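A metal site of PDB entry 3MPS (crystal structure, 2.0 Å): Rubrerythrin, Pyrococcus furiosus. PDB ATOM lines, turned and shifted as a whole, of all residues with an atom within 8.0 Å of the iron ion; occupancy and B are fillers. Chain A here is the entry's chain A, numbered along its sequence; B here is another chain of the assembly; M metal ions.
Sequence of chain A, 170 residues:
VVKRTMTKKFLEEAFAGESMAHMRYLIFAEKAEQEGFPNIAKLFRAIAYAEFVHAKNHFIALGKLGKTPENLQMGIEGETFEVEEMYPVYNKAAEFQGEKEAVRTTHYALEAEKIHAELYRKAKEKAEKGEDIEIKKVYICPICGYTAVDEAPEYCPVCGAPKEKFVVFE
SG of Cys 159 lies close to N of Ala 161, 3.5 Å away. SG of Cys 141 lies close to N of Ile 143. The side-chain sulfur of Cys 156 sits close to the backbone NH of Val 158. SG of Cys 144 sits close to N of Tyr 146 (3.5 Å). O of Tyr 146 is in hydrogen-bond range of N of Cys 141, at 2.9 Å. The backbone NH of Cys 156 lies within hydrogen-bond range of the backbone carbonyl oxygen of Ala 161 (2.8 Å).
Four residues have an atom within 4 Å of the iron ion: Cys 141, Cys 144, Cys 156 and Cys 159.
The iron ion is bound by the side-chain sulfur (SG) of Cys 144 (2.3 Å), the side-chain sulfur (SG) of Cys 159 (2.3 Å), the side-chain sulfur (SG) of Cys 141 (2.3 Å) and the side-chain sulfur (SG) of Cys 156 (2.3 Å). The iron ion has four donor atoms within binding distance.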
ATOM      1  N   TYR A 108     -11.026  -2.675  23.604  1.00  0.00           N
ATOM      2  CA  TYR A 108     -10.673  -2.789  22.178  1.00  0.00           C
ATOM      3  C   TYR A 108     -11.482  -3.883  21.495  1.00  0.00           C
ATOM      4  O   TYR A 108     -12.066  -3.675  20.429  1.00  0.00           O
ATOM      5  CB  TYR A 108      -9.184  -3.117  22.019  1.00  0.00           C
ATOM      6  CG  TYR A 108      -8.224  -1.952  22.177  1.00  0.00           C
ATOM      7  CD1 TYR A 108      -8.679  -0.632  22.287  1.00  0.00           C
ATOM      8  CD2 TYR A 108      -6.853  -2.183  22.197  1.00  0.00           C
ATOM      9  CE1 TYR A 108      -7.785   0.418  22.431  1.00  0.00           C
ATOM     10  CE2 TYR A 108      -5.962  -1.154  22.335  1.00  0.00           C
ATOM     11  CZ  TYR A 108      -6.420   0.143  22.461  1.00  0.00           C
ATOM     12  OH  TYR A 108      -5.503   1.150  22.584  1.00  0.00           O
ATOM     13  N   ALA A 112     -14.341  -3.701  18.639  1.00  0.00           N
ATOM     14  CA  ALA A 112     -13.805  -4.198  17.369  1.00  0.00           C
ATOM     15  C   ALA A 112     -14.450  -5.493  16.851  1.00  0.00           C
ATOM     16  O   ALA A 112     -14.322  -5.808  15.665  1.00  0.00           O
ATOM     17  CB  ALA A 112     -12.291  -4.356  17.456  1.00  0.00           C
ATOM     18  N   ILE A 140      -7.257  -4.309   8.782  1.00  0.00           N
ATOM     19  CA  ILE A 140      -7.252  -4.608  10.218  1.00  0.00           C
ATOM     20  C   ILE A 140      -6.261  -3.712  10.950  1.00  0.00           C
ATOM     21  O   ILE A 140      -5.074  -3.661  10.595  1.00  0.00           O
ATOM     22  CB  ILE A 140      -6.881  -6.099  10.565  1.00  0.00           C
ATOM     23  CG1 ILE A 140      -7.521  -7.122   9.595  1.00  0.00           C
ATOM     24  CG2 ILE A 140      -7.150  -6.384  12.059  1.00  0.00           C
ATOM     25  CD1 ILE A 140      -9.039  -7.301   9.660  1.00  0.00           C
ATOM     26  N   CYS A 141      -6.754  -3.017  11.965  1.00  0.00           N
ATOM     27  CA  CYS A 141      -5.901  -2.258  12.859  1.00  0.00           C
ATOM     28  C   CYS A 141      -4.978  -3.185  13.685  1.00  0.00           C
ATOM     29  O   CYS A 141      -5.457  -4.056  14.424  1.00  0.00           O
ATOM     30  CB  CYS A 141      -6.708  -1.342  13.775  1.00  0.00           C
ATOM     31  SG  CYS A 141      -5.636  -0.312  14.796  1.00  0.00           S
ATOM     32  N   PRO A 142      -3.654  -2.991  13.559  1.00  0.00           N
ATOM     33  CA  PRO A 142      -2.685  -3.813  14.295  1.00  0.00           C
ATOM     34  C   PRO A 142      -2.692  -3.576  15.822  1.00  0.00           C
ATOM     35  O   PRO A 142      -2.097  -4.371  16.578  1.00  0.00           O
ATOM     36  CB  PRO A 142      -1.338  -3.412  13.677  1.00  0.00           C
ATOM     37  CG  PRO A 142      -1.572  -2.003  13.152  1.00  0.00           C
ATOM     38  CD  PRO A 142      -2.990  -1.990  12.681  1.00  0.00           C
ATOM     39  N   ILE A 143      -3.363  -2.513  16.267  1.00  0.00           N
ATOM     40  CA  ILE A 143      -3.320  -2.106  17.687  1.00  0.00           C
ATOM     41  C   ILE A 143      -4.485  -2.721  18.442  1.00  0.00           C
ATOM     42  O   ILE A 143      -4.301  -3.339  19.497  1.00  0.00           O
ATOM     43  CB  ILE A 143      -3.360  -0.531  17.838  1.00  0.00           C
ATOM     44  CG1 ILE A 143      -2.122   0.131  17.200  1.00  0.00           C
ATOM     45  CG2 ILE A 143      -3.558  -0.109  19.298  1.00  0.00           C
ATOM     46  CD1 ILE A 143      -0.773  -0.169  17.869  1.00  0.00           C
ATOM     47  N   CYS A 144      -5.675  -2.567  17.878  1.00  0.00           N
ATOM     48  CA  CYS A 144      -6.906  -2.884  18.563  1.00  0.00           C
ATOM     49  C   CYS A 144      -7.833  -3.810  17.777  1.00  0.00           C
ATOM     50  O   CYS A 144      -8.934  -4.092  18.238  1.00  0.00           O
ATOM     51  CB  CYS A 144      -7.674  -1.586  18.794  1.00  0.00           C
ATOM     52  SG  CYS A 144      -8.319  -1.009  17.241  1.00  0.00           S
ATOM     53  N   GLY A 145      -7.410  -4.242  16.590  1.00  0.00           N
ATOM     54  CA  GLY A 145      -8.152  -5.269  15.841  1.00  0.00           C
ATOM     55  C   GLY A 145      -9.362  -4.783  15.067  1.00  0.00           C
ATOM     56  O   GLY A 145     -10.033  -5.571  14.387  1.00  0.00           O
ATOM     57  N   TYR A 146      -9.654  -3.472  15.144  1.00  0.00           N
ATOM     58  CA  TYR A 146     -10.760  -2.868  14.359  1.00  0.00           C
ATOM     59  C   TYR A 146     -10.695  -3.344  12.909  1.00  0.00           C
ATOM     60  O   TYR A 146      -9.625  -3.443  12.335  1.00  0.00           O
ATOM     61  CB  TYR A 146     -10.757  -1.329  14.454  1.00  0.00           C
ATOM     62  CG  TYR A 146     -11.612  -0.649  13.401  1.00  0.00           C
ATOM     63  CD1 TYR A 146     -11.046  -0.217  12.207  1.00  0.00           C
ATOM     64  CD2 TYR A 146     -12.982  -0.463  13.589  1.00  0.00           C
ATOM     65  CE1 TYR A 146     -11.806   0.394  11.210  1.00  0.00           C
ATOM     66  CE2 TYR A 146     -13.763   0.152  12.583  1.00  0.00           C
ATOM     67  CZ  TYR A 146     -13.157   0.575  11.407  1.00  0.00           C
ATOM     68  OH  TYR A 146     -13.886   1.176  10.401  1.00  0.00           O
ATOM     69  N   THR A 147     -11.868  -3.637  12.346  1.00  0.00           N
ATOM     70  CA  THR A 147     -12.002  -4.378  11.102  1.00  0.00           C
ATOM     71  C   THR A 147     -12.938  -3.677  10.139  1.00  0.00           C
ATOM     72  O   THR A 147     -14.074  -3.365  10.498  1.00  0.00           O
ATOM     73  CB  THR A 147     -12.558  -5.789  11.371  1.00  0.00           C
ATOM     74  OG1 THR A 147     -11.604  -6.534  12.139  1.00  0.00           O
ATOM     75  CG2 THR A 147     -12.874  -6.542  10.077  1.00  0.00           C
ATOM     76  N   TYR A 155      -8.904   7.534  10.476  1.00  0.00           N
ATOM     77  CA  TYR A 155      -8.342   7.084  11.762  1.00  0.00           C
ATOM     78  C   TYR A 155      -9.198   5.958  12.331  1.00  0.00           C
ATOM     79  O   TYR A 155     -10.406   5.936  12.131  1.00  0.00           O
ATOM     80  CB  TYR A 155      -8.201   8.275  12.733  1.00  0.00           C
ATOM     81  CG  TYR A 155      -7.353   9.367  12.152  1.00  0.00           C
ATOM     82  CD1 TYR A 155      -5.970   9.325  12.244  1.00  0.00           C
ATOM     83  CD2 TYR A 155      -7.945  10.433  11.447  1.00  0.00           C
ATOM     84  CE1 TYR A 155      -5.184  10.313  11.677  1.00  0.00           C
ATOM     85  CE2 TYR A 155      -7.153  11.434  10.863  1.00  0.00           C
ATOM     86  CZ  TYR A 155      -5.774  11.368  10.993  1.00  0.00           C
ATOM     87  OH  TYR A 155      -4.952  12.346  10.431  1.00  0.00           O
ATOM     88  N   CYS A 156      -8.549   5.017  13.002  1.00  0.00           N
ATOM     89  CA  CYS A 156      -9.263   3.920  13.661  1.00  0.00           C
ATOM     90  C   CYS A 156     -10.182   4.498  14.730  1.00  0.00           C
ATOM     91  O   CYS A 156      -9.717   5.241  15.605  1.00  0.00           O
ATOM     92  CB  CYS A 156      -8.268   2.955  14.298  1.00  0.00           C
ATOM     93  SG  CYS A 156      -9.018   1.579  15.197  1.00  0.00           S
ATOM     94  N   PRO A 157     -11.487   4.153  14.671  1.00  0.00           N
ATOM     95  CA  PRO A 157     -12.507   4.719  15.571  1.00  0.00           C
ATOM     96  C   PRO A 157     -12.324   4.256  17.004  1.00  0.00           C
ATOM     97  O   PRO A 157     -12.848   4.882  17.942  1.00  0.00           O
ATOM     98  CB  PRO A 157     -13.827   4.159  15.021  1.00  0.00           C
ATOM     99  CG  PRO A 157     -13.485   3.509  13.710  1.00  0.00           C
ATOM    100  CD  PRO A 157     -12.061   3.169  13.732  1.00  0.00           C
ATOM    101  N   VAL A 158     -11.568   3.182  17.161  1.00  0.00           N
ATOM    102  CA  VAL A 158     -11.354   2.507  18.437  1.00  0.00           C
ATOM    103  C   VAL A 158     -10.121   3.083  19.130  1.00  0.00           C
ATOM    104  O   VAL A 158     -10.217   3.528  20.257  1.00  0.00           O
ATOM    105  CB  VAL A 158     -11.188   0.986  18.226  1.00  0.00           C
ATOM    106  CG1 VAL A 158     -10.939   0.258  19.530  1.00  0.00           C
ATOM    107  CG2 VAL A 158     -12.415   0.415  17.480  1.00  0.00           C
ATOM    108  N   CYS A 159      -8.980   3.088  18.443  1.00  0.00           N
ATOM    109  CA  CYS A 159      -7.726   3.485  19.083  1.00  0.00           C
ATOM    110  C   CYS A 159      -7.079   4.763  18.556  1.00  0.00           C
ATOM    111  O   CYS A 159      -6.114   5.251  19.137  1.00  0.00           O
ATOM    112  CB  CYS A 159      -6.709   2.336  19.070  1.00  0.00           C
ATOM    113  SG  CYS A 159      -5.859   2.094  17.503  1.00  0.00           S
ATOM    114  N   GLY A 160      -7.589   5.282  17.437  1.00  0.00           N
ATOM    115  CA  GLY A 160      -7.043   6.500  16.845  1.00  0.00           C
ATOM    116  C   GLY A 160      -5.900   6.313  15.876  1.00  0.00           C
ATOM    117  O   GLY A 160      -5.423   7.298  15.311  1.00  0.00           O
ATOM    118  N   ALA A 161      -5.470   5.076  15.646  1.00  0.00           N
ATOM    119  CA  ALA A 161      -4.357   4.814  14.725  1.00  0.00           C
ATOM    120  C   ALA A 161      -4.683   5.211  13.284  1.00  0.00           C
ATOM    121  O   ALA A 161      -5.782   4.896  12.788  1.00  0.00           O
ATOM    122  CB  ALA A 161      -3.933   3.347  14.784  1.00  0.00           C
ATOM    123  N   PRO A 162      -3.751   5.926  12.616  1.00  0.00           N
ATOM    124  CA  PRO A 162      -3.978   6.269  11.213  1.00  0.00           C
ATOM    125  C   PRO A 162      -4.088   5.041  10.308  1.00  0.00           C
ATOM    126  O   PRO A 162      -3.438   4.022  10.561  1.00  0.00           O
ATOM    127  CB  PRO A 162      -2.751   7.110  10.839  1.00  0.00           C
ATOM    128  CG  PRO A 162      -1.728   6.891  11.933  1.00  0.00           C
ATOM    129  CD  PRO A 162      -2.483   6.461  13.145  1.00  0.00           C
ATOM    130  N   LYS A 165      -1.400   2.676   9.136  1.00  0.00           N
ATOM    131  CA  LYS A 165      -0.995   1.620  10.080  1.00  0.00           C
ATOM    132  C   LYS A 165      -1.711   0.286   9.826  1.00  0.00           C
ATOM    133  O   LYS A 165      -1.166  -0.781  10.140  1.00  0.00           O
ATOM    134  CB  LYS A 165      -1.270   2.051  11.525  1.00  0.00           C
ATOM    135  CG  LYS A 165      -0.519   3.297  12.007  1.00  0.00           C
ATOM    136  CD  LYS A 165      -0.578   3.371  13.540  1.00  0.00           C
ATOM    137  CE  LYS A 165       0.231   4.525  14.111  1.00  0.00           C
ATOM    138  NZ  LYS A 165       0.363   4.399  15.594  1.00  0.00           N
ATOM    139  N   PHE A 166      -2.915   0.360   9.283  1.00  0.00           N
ATOM    140  CA  PHE A 166      -3.760  -0.815   9.033  1.00  0.00           C
ATOM    141  C   PHE A 166      -3.111  -1.880   8.174  1.00  0.00           C
ATOM    142  O   PHE A 166      -2.453  -1.577   7.170  1.00  0.00           O
ATOM    143  CB  PHE A 166      -5.082  -0.393   8.382  1.00  0.00           C
ATOM    144  CG  PHE A 166      -5.917   0.519   9.225  1.00  0.00           C
ATOM    145  CD1 PHE A 166      -5.467   0.971  10.473  1.00  0.00           C
ATOM    146  CD2 PHE A 166      -7.160   0.943   8.787  1.00  0.00           C
ATOM    147  CE1 PHE A 166      -6.243   1.811  11.250  1.00  0.00           C
ATOM    148  CE2 PHE A 166      -7.940   1.783   9.550  1.00  0.00           C
ATOM    149  CZ  PHE A 166      -7.487   2.226  10.775  1.00  0.00           C
ATOM    150  N   VAL B  53      -4.562 -10.222  17.059  1.00  0.00           N
ATOM    151  CA  VAL B  53      -4.382  -8.925  17.707  1.00  0.00           C
ATOM    152  C   VAL B  53      -4.923  -8.934  19.146  1.00  0.00           C
ATOM    153  O   VAL B  53      -4.237  -8.503  20.076  1.00  0.00           O
ATOM    154  CB  VAL B  53      -4.998  -7.754  16.887  1.00  0.00           C
ATOM    155  CG1 VAL B  53      -4.866  -6.427  17.665  1.00  0.00           C
ATOM    156  CG2 VAL B  53      -4.312  -7.611  15.563  1.00  0.00           C
HETATM  157 FE    FE M   1      -7.152   0.685  16.226  1.00  0.00          FE
